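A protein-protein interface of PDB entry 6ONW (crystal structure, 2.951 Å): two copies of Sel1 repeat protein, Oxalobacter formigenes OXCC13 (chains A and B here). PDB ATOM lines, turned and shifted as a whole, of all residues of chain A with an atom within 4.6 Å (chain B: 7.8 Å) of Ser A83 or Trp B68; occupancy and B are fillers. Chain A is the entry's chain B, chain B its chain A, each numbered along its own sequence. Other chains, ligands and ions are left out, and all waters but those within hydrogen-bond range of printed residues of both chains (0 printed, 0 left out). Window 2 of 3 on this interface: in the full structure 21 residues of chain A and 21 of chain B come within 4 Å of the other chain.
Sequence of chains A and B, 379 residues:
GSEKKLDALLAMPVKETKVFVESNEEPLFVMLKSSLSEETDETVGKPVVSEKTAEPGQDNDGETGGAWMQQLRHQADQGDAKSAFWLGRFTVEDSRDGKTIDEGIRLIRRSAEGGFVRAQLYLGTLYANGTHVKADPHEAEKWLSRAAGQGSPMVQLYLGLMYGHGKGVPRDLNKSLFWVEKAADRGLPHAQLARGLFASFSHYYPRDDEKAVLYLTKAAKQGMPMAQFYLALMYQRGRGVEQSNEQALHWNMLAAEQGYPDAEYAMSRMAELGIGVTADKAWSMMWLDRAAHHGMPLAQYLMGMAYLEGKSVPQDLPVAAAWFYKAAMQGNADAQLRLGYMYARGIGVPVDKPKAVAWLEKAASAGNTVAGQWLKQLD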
ATOM      1  N   TRP A  68      23.668  21.737  17.390  1.00  0.00           N
ATOM      2  CA  TRP A  68      23.253  21.496  18.767  1.00  0.00           C
ATOM      3  C   TRP A  68      24.279  22.022  19.760  1.00  0.00           C
ATOM      4  O   TRP A  68      23.915  22.430  20.869  1.00  0.00           O
ATOM      5  CB  TRP A  68      23.020  20.003  18.995  1.00  0.00           C
ATOM      6  CG  TRP A  68      24.274  19.190  18.913  1.00  0.00           C
ATOM      7  CD1 TRP A  68      24.806  18.614  17.797  1.00  0.00           C
ATOM      8  CD2 TRP A  68      25.161  18.867  19.992  1.00  0.00           C
ATOM      9  NE1 TRP A  68      25.967  17.952  18.114  1.00  0.00           N
ATOM     10  CE2 TRP A  68      26.207  18.093  19.455  1.00  0.00           C
ATOM     11  CE3 TRP A  68      25.170  19.160  21.359  1.00  0.00           C
ATOM     12  CZ2 TRP A  68      27.250  17.605  20.238  1.00  0.00           C
ATOM     13  CZ3 TRP A  68      26.208  18.674  22.134  1.00  0.00           C
ATOM     14  CH2 TRP A  68      27.233  17.905  21.572  1.00  0.00           C
ATOM     15  N   GLN A  71      23.945  25.777  20.246  1.00  0.00           N
ATOM     16  CA  GLN A  71      22.857  25.982  21.196  1.00  0.00           C
ATOM     17  C   GLN A  71      23.303  25.651  22.614  1.00  0.00           C
ATOM     18  O   GLN A  71      22.932  26.347  23.567  1.00  0.00           O
ATOM     19  CB  GLN A  71      21.648  25.133  20.804  1.00  0.00           C
ATOM     20  CG  GLN A  71      20.791  25.725  19.696  1.00  0.00           C
ATOM     21  CD  GLN A  71      19.919  26.868  20.182  1.00  0.00           C
ATOM     22  OE1 GLN A  71      19.832  27.133  21.383  1.00  0.00           O
ATOM     23  NE2 GLN A  71      19.266  27.552  19.250  1.00  0.00           N
ATOM     24  N   LEU A  72      24.102  24.593  22.772  1.00  0.00           N
ATOM     25  CA  LEU A  72      24.568  24.203  24.097  1.00  0.00           C
ATOM     26  C   LEU A  72      25.596  25.190  24.636  1.00  0.00           C
ATOM     27  O   LEU A  72      25.557  25.552  25.817  1.00  0.00           O
ATOM     28  CB  LEU A  72      25.152  22.792  24.048  1.00  0.00           C
ATOM     29  CG  LEU A  72      25.778  22.251  25.334  1.00  0.00           C
ATOM     30  CD1 LEU A  72      24.751  22.211  26.445  1.00  0.00           C
ATOM     31  CD2 LEU A  72      26.367  20.870  25.100  1.00  0.00           C
ATOM     32  N   GLN A  75      24.005  28.415  26.137  1.00  0.00           N
ATOM     33  CA  GLN A  75      23.504  28.277  27.500  1.00  0.00           C
ATOM     34  C   GLN A  75      24.646  28.320  28.507  1.00  0.00           C
ATOM     35  O   GLN A  75      24.509  28.900  29.590  1.00  0.00           O
ATOM     36  CB  GLN A  75      22.717  26.973  27.643  1.00  0.00           C
ATOM     37  CG  GLN A  75      21.682  26.736  26.553  1.00  0.00           C
ATOM     38  CD  GLN A  75      20.496  27.673  26.651  1.00  0.00           C
ATOM     39  OE1 GLN A  75      19.985  27.932  27.740  1.00  0.00           O
ATOM     40  NE2 GLN A  75      20.052  28.189  25.510  1.00  0.00           N
ATOM     41  N   ALA A  76      25.786  27.720  28.159  1.00  0.00           N
ATOM     42  CA  ALA A  76      26.921  27.687  29.075  1.00  0.00           C
ATOM     43  C   ALA A  76      27.487  29.081  29.310  1.00  0.00           C
ATOM     44  O   ALA A  76      27.869  29.419  30.436  1.00  0.00           O
ATOM     45  CB  ALA A  76      28.003  26.756  28.532  1.00  0.00           C
ATOM     46  N   ASP A  80      24.077  28.967  32.711  1.00  0.00           N
ATOM     47  CA  ASP A  80      23.565  27.607  32.882  1.00  0.00           C
ATOM     48  C   ASP A  80      24.723  26.688  33.252  1.00  0.00           C
ATOM     49  O   ASP A  80      25.455  26.208  32.385  1.00  0.00           O
ATOM     50  CB  ASP A  80      22.862  27.134  31.615  1.00  0.00           C
ATOM     51  CG  ASP A  80      22.047  25.873  31.836  1.00  0.00           C
ATOM     52  OD1 ASP A  80      22.001  25.380  32.983  1.00  0.00           O
ATOM     53  OD2 ASP A  80      21.447  25.375  30.860  1.00  0.00           O
ATOM     54  N   ALA A  81      24.891  26.439  34.554  1.00  0.00           N
ATOM     55  CA  ALA A  81      26.008  25.622  35.016  1.00  0.00           C
ATOM     56  C   ALA A  81      25.850  24.162  34.612  1.00  0.00           C
ATOM     57  O   ALA A  81      26.851  23.458  34.439  1.00  0.00           O
ATOM     58  CB  ALA A  81      26.156  25.743  36.533  1.00  0.00           C
ATOM     59  N   LYS A  82      24.611  23.687  34.463  1.00  0.00           N
ATOM     60  CA  LYS A  82      24.402  22.319  34.002  1.00  0.00           C
ATOM     61  C   LYS A  82      24.882  22.146  32.567  1.00  0.00           C
ATOM     62  O   LYS A  82      25.558  21.160  32.246  1.00  0.00           O
ATOM     63  CB  LYS A  82      22.926  21.940  34.123  1.00  0.00           C
ATOM     64  CG  LYS A  82      22.404  21.898  35.548  1.00  0.00           C
ATOM     65  CD  LYS A  82      20.918  21.572  35.576  1.00  0.00           C
ATOM     66  CE  LYS A  82      20.383  21.534  36.998  1.00  0.00           C
ATOM     67  NZ  LYS A  82      21.058  20.488  37.817  1.00  0.00           N
ATOM     68  N   SER A  83      24.549  23.097  31.692  1.00  0.00           N
ATOM     69  CA  SER A  83      24.993  23.015  30.305  1.00  0.00           C
ATOM     70  C   SER A  83      26.505  23.174  30.198  1.00  0.00           C
ATOM     71  O   SER A  83      27.145  22.522  29.366  1.00  0.00           O
ATOM     72  CB  SER A  83      24.279  24.069  29.464  1.00  0.00           C
ATOM     73  OG  SER A  83      22.884  23.829  29.429  1.00  0.00           O
ATOM     74  N   ALA A  84      27.093  24.039  31.030  1.00  0.00           N
ATOM     75  CA  ALA A  84      28.542  24.201  31.014  1.00  0.00           C
ATOM     76  C   ALA A  84      29.250  22.925  31.447  1.00  0.00           C
ATOM     77  O   ALA A  84      30.351  22.632  30.967  1.00  0.00           O
ATOM     78  CB  ALA A  84      28.953  25.369  31.910  1.00  0.00           C
ATOM     79  N   PHE A  85      28.637  22.154  32.345  1.00  0.00           N
ATOM     80  CA  PHE A  85      29.241  20.893  32.758  1.00  0.00           C
ATOM     81  C   PHE A  85      29.095  19.830  31.678  1.00  0.00           C
ATOM     82  O   PHE A  85      30.041  19.082  31.405  1.00  0.00           O
ATOM     83  CB  PHE A  85      28.620  20.415  34.068  1.00  0.00           C
ATOM     84  CG  PHE A  85      29.056  19.039  34.474  1.00  0.00           C
ATOM     85  CD1 PHE A  85      30.315  18.827  35.009  1.00  0.00           C
ATOM     86  CD2 PHE A  85      28.209  17.954  34.321  1.00  0.00           C
ATOM     87  CE1 PHE A  85      30.722  17.562  35.382  1.00  0.00           C
ATOM     88  CE2 PHE A  85      28.609  16.688  34.692  1.00  0.00           C
ATOM     89  CZ  PHE A  85      29.867  16.491  35.224  1.00  0.00           C
ATOM     90  N   TRP A  86      27.917  19.746  31.053  1.00  0.00           N
ATOM     91  CA  TRP A  86      27.699  18.742  30.017  1.00  0.00           C
ATOM     92  C   TRP A  86      28.628  18.973  28.832  1.00  0.00           C
ATOM     93  O   TRP A  86      29.251  18.036  28.322  1.00  0.00           O
ATOM     94  CB  TRP A  86      26.237  18.757  29.570  1.00  0.00           C
ATOM     95  CG  TRP A  86      25.760  17.448  29.009  1.00  0.00           C
ATOM     96  CD1 TRP A  86      25.038  16.492  29.663  1.00  0.00           C
ATOM     97  CD2 TRP A  86      25.972  16.951  27.681  1.00  0.00           C
ATOM     98  NE1 TRP A  86      24.785  15.433  28.825  1.00  0.00           N
ATOM     99  CE2 TRP A  86      25.348  15.689  27.603  1.00  0.00           C
ATOM    100  CE3 TRP A  86      26.627  17.450  26.550  1.00  0.00           C
ATOM    101  CZ2 TRP A  86      25.362  14.921  26.440  1.00  0.00           C
ATOM    102  CZ3 TRP A  86      26.639  16.684  25.398  1.00  0.00           C
ATOM    103  CH2 TRP A  86      26.011  15.433  25.352  1.00  0.00           C
ATOM    104  N   LEU A  87      28.738  20.226  28.382  1.00  0.00           N
ATOM    105  CA  LEU A  87      29.649  20.543  27.289  1.00  0.00           C
ATOM    106  C   LEU A  87      31.103  20.394  27.721  1.00  0.00           C
ATOM    107  O   LEU A  87      31.936  19.895  26.955  1.00  0.00           O
ATOM    108  CB  LEU A  87      29.387  21.961  26.781  1.00  0.00           C
ATOM    109  CG  LEU A  87      30.303  22.466  25.668  1.00  0.00           C
ATOM    110  CD1 LEU A  87      30.173  21.590  24.433  1.00  0.00           C
ATOM    111  CD2 LEU A  87      29.993  23.917  25.336  1.00  0.00           C
ATOM    112  N   GLY B  66      16.941  20.673  27.579  1.00  0.00           N
ATOM    113  CA  GLY B  66      16.645  21.890  26.845  1.00  0.00           C
ATOM    114  C   GLY B  66      16.420  21.658  25.364  1.00  0.00           C
ATOM    115  O   GLY B  66      16.028  20.566  24.952  1.00  0.00           O
ATOM    116  N   ALA B  67      16.669  22.693  24.558  1.00  0.00           N
ATOM    117  CA  ALA B  67      16.494  22.568  23.115  1.00  0.00           C
ATOM    118  C   ALA B  67      17.712  21.954  22.443  1.00  0.00           C
ATOM    119  O   ALA B  67      17.580  21.322  21.389  1.00  0.00           O
ATOM    120  CB  ALA B  67      16.191  23.934  22.499  1.00  0.00           C
ATOM    121  N   TRP B  68      18.899  22.126  23.031  1.00  0.00           N
ATOM    122  CA  TRP B  68      20.108  21.561  22.442  1.00  0.00           C
ATOM    123  C   TRP B  68      20.084  20.040  22.458  1.00  0.00           C
ATOM    124  O   TRP B  68      20.669  19.403  21.574  1.00  0.00           O
ATOM    125  CB  TRP B  68      21.344  22.074  23.181  1.00  0.00           C
ATOM    126  CG  TRP B  68      21.395  21.662  24.621  1.00  0.00           C
ATOM    127  CD1 TRP B  68      20.901  22.351  25.690  1.00  0.00           C
ATOM    128  CD2 TRP B  68      21.974  20.461  25.151  1.00  0.00           C
ATOM    129  NE1 TRP B  68      21.136  21.656  26.851  1.00  0.00           N
ATOM    130  CE2 TRP B  68      21.792  20.493  26.548  1.00  0.00           C
ATOM    131  CE3 TRP B  68      22.625  19.365  24.580  1.00  0.00           C
ATOM    132  CZ2 TRP B  68      22.241  19.471  27.381  1.00  0.00           C
ATOM    133  CZ3 TRP B  68      23.070  18.351  25.408  1.00  0.00           C
ATOM    134  CH2 TRP B  68      22.878  18.412  26.794  1.00  0.00           C
ATOM    135  N   MET B  69      19.425  19.443  23.445  1.00  0.00           N
ATOM    136  CA  MET B  69      19.352  17.993  23.541  1.00  0.00           C
ATOM    137  C   MET B  69      18.398  17.429  22.491  1.00  0.00           C
ATOM    138  O   MET B  69      18.604  16.326  21.982  1.00  0.00           O
ATOM    139  CB  MET B  69      18.923  17.571  24.947  1.00  0.00           C
ATOM    140  CG  MET B  69      18.863  16.068  25.150  1.00  0.00           C
ATOM    141  SD  MET B  69      18.812  15.561  27.029  1.00  0.00           S
ATOM    142  CE  MET B  69      20.692  15.809  27.470  1.00  0.00           C
ATOM    143  N   GLN B  70      17.352  18.193  22.163  1.00  0.00           N
ATOM    144  CA  GLN B  70      16.460  17.783  21.084  1.00  0.00           C
ATOM    145  C   GLN B  70      17.184  17.798  19.743  1.00  0.00           C
ATOM    146  O   GLN B  70      17.027  16.875  18.934  1.00  0.00           O
ATOM    147  CB  GLN B  70      15.228  18.686  21.039  1.00  0.00           C
ATOM    148  CG  GLN B  70      14.381  18.651  22.299  1.00  0.00           C
ATOM    149  CD  GLN B  70      13.109  19.460  22.160  1.00  0.00           C
ATOM    150  OE1 GLN B  70      12.566  19.602  21.065  1.00  0.00           O
ATOM    151  NE2 GLN B  70      12.628  20.003  23.274  1.00  0.00           N
ATOM    152  N   GLN B  71      17.978  18.842  19.491  1.00  0.00           N
ATOM    153  CA  GLN B  71      18.801  18.872  18.286  1.00  0.00           C
ATOM    154  C   GLN B  71      19.811  17.732  18.287  1.00  0.00           C
ATOM    155  O   GLN B  71      20.066  17.118  17.245  1.00  0.00           O
ATOM    156  CB  GLN B  71      19.518  20.219  18.174  1.00  0.00           C
ATOM    157  CG  GLN B  71      18.601  21.410  17.946  1.00  0.00           C
ATOM    158  CD  GLN B  71      18.085  21.483  16.524  1.00  0.00           C
ATOM    159  OE1 GLN B  71      18.620  20.835  15.623  1.00  0.00           O
ATOM    160  NE2 GLN B  71      17.040  22.275  16.314  1.00  0.00           N
ATOM    161  N   LEU B  72      20.388  17.431  19.453  1.00  0.00           N
ATOM    162  CA  LEU B  72      21.386  16.369  19.542  1.00  0.00           C
ATOM    163  C   LEU B  72      20.770  15.002  19.268  1.00  0.00           C
ATOM    164  O   LEU B  72      21.347  14.192  18.533  1.00  0.00           O
ATOM    165  CB  LEU B  72      22.050  16.395  20.918  1.00  0.00           C
ATOM    166  CG  LEU B  72      23.070  15.295  21.212  1.00  0.00           C
ATOM    167  CD1 LEU B  72      24.227  15.367  20.236  1.00  0.00           C
ATOM    168  CD2 LEU B  72      23.567  15.399  22.644  1.00  0.00           C
ATOM    169  N   ARG B  73      19.602  14.725  19.853  1.00  0.00           N
ATOM    170  CA  ARG B  73      18.942  13.444  19.618  1.00  0.00           C
ATOM    171  C   ARG B  73      18.525  13.302  18.161  1.00  0.00           C
ATOM    172  O   ARG B  73      18.586  12.205  17.593  1.00  0.00           O
ATOM    173  CB  ARG B  73      17.731  13.303  20.538  1.00  0.00           C
ATOM    174  CG  ARG B  73      17.026  11.961  20.444  1.00  0.00           C
ATOM    175  CD  ARG B  73      15.835  11.911  21.384  1.00  0.00           C
ATOM    176  NE  ARG B  73      16.185  12.382  22.720  1.00  0.00           N
ATOM    177  CZ  ARG B  73      16.696  11.612  23.674  1.00  0.00           C
ATOM    178  NH1 ARG B  73      16.915  10.324  23.444  1.00  0.00           N
ATOM    179  NH2 ARG B  73      16.988  12.129  24.860  1.00  0.00           N
ATOM    180  N   HIS B  74      18.098  14.404  17.539  1.00  0.00           N
ATOM    181  CA  HIS B  74      17.714  14.363  16.133  1.00  0.00           C
ATOM    182  C   HIS B  74      18.889  13.953  15.254  1.00  0.00           C
ATOM    183  O   HIS B  74      18.714  13.230  14.265  1.00  0.00           O
ATOM    184  CB  HIS B  74      17.165  15.725  15.707  1.00  0.00           C
ATOM    185  CG  HIS B  74      16.696  15.772  14.287  1.00  0.00           C
ATOM    186  ND1 HIS B  74      15.840  14.833  13.753  1.00  0.00           N
ATOM    187  CD2 HIS B  74      16.960  16.652  13.291  1.00  0.00           C
ATOM    188  CE1 HIS B  74      15.600  15.129  12.488  1.00  0.00           C
ATOM    189  NE2 HIS B  74      16.268  16.228  12.183  1.00  0.00           N
ATOM    190  N   GLN B  75      20.100  14.400  15.602  1.00  0.00           N
ATOM    191  CA  GLN B  75      21.285  13.971  14.867  1.00  0.00           C
ATOM    192  C   GLN B  75      21.507  12.472  15.018  1.00  0.00           C
ATOM    193  O   GLN B  75      21.833  11.782  14.045  1.00  0.00           O
ATOM    194  CB  GLN B  75      22.514  14.741  15.353  1.00  0.00           C
ATOM    195  CG  GLN B  75      22.389  16.251  15.260  1.00  0.00           C
ATOM    196  CD  GLN B  75      22.281  16.742  13.832  1.00  0.00           C
ATOM    197  OE1 GLN B  75      21.313  17.411  13.467  1.00  0.00           O
ATOM    198  NE2 GLN B  75      23.278  16.418  13.018  1.00  0.00           N
ATOM    199  N   LEU B  87      25.409  11.131  23.801  1.00  0.00           N
ATOM    200  CA  LEU B  87      24.123  11.416  24.430  1.00  0.00           C
ATOM    201  C   LEU B  87      23.632  10.219  25.233  1.00  0.00           C
ATOM    202  O   LEU B  87      23.151  10.374  26.361  1.00  0.00           O
ATOM    203  CB  LEU B  87      23.090  11.816  23.377  1.00  0.00           C
ATOM    204  CG  LEU B  87      21.661  12.013  23.892  1.00  0.00           C
ATOM    205  CD1 LEU B  87      21.605  13.140  24.909  1.00  0.00           C
ATOM    206  CD2 LEU B  87      20.697  12.274  22.747  1.00  0.00           C
ATOM    207  N   PHE B  90      25.971   9.633  28.469  1.00  0.00           N
ATOM    208  CA  PHE B  90      25.701  10.631  29.495  1.00  0.00           C
ATOM    209  C   PHE B  90      24.258  10.598  29.979  1.00  0.00           C
ATOM    210  O   PHE B  90      23.955  11.212  31.006  1.00  0.00           O
ATOM    211  CB  PHE B  90      26.057  12.024  28.972  1.00  0.00           C
ATOM    212  CG  PHE B  90      27.528  12.213  28.705  1.00  0.00           C
ATOM    213  CD1 PHE B  90      28.470  11.462  29.389  1.00  0.00           C
ATOM    214  CD2 PHE B  90      27.966  13.135  27.771  1.00  0.00           C
ATOM    215  CE1 PHE B  90      29.821  11.630  29.149  1.00  0.00           C
ATOM    216  CE2 PHE B  90      29.318  13.307  27.526  1.00  0.00           C
ATOM    217  CZ  PHE B  90      30.244  12.553  28.217  1.00  0.00           C
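Trp B68 touches five residues of chain A. Of the printed residues of chain A, Gln B71 touches Trp A68 (3.6 Å). Of the printed residues of chain B, Trp A86 touches Trp B68, Leu B72 and Phe B90. Asp A80 touches none of the printed residues of chain B. Gln B70 touches none of the printed residues of chain A. The nearest residue of chain A that does not touch Trp B68 is Gln A75 (4.5 Å).
Among the printed residues, pairs that only touch across the chains: Trp A68 with Trp B68, Trp A68 with Gln B71, Trp A68 with Leu B72, Gln A71 with Trp B68, Leu A72 with Trp B68, Ser A83 with Trp B68, Trp A86 with Trp B68, Trp A86 with Leu B72 and Trp A86 with Phe B90.
The side-chain carboxylate (OD2) of Asp A80 sits at hydrogen-bond distance from the side-chain hydroxyl (OG) of Ser A83 (2.6 Å).
Along chain B the printed residues that touch a printed residue of chain A span positions 68 to 90. Of the 13 printed residues of chain A, 5 touch a printed residue of chain B. Among the printed residues, 9 pairs touch across the chains.
Trp B68 touches its own counterpart, Trp A68. Trp A68 touches Gln B71, and with the chains exchanged Gln A71 touches Trp B68. Trp A68 touches Leu B72, and with the chains exchanged Leu A72 touches Trp B68. Of the 9 pairs that touch across the chains among the printed residues, 5 have their exchanged pair printed and touching as well.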
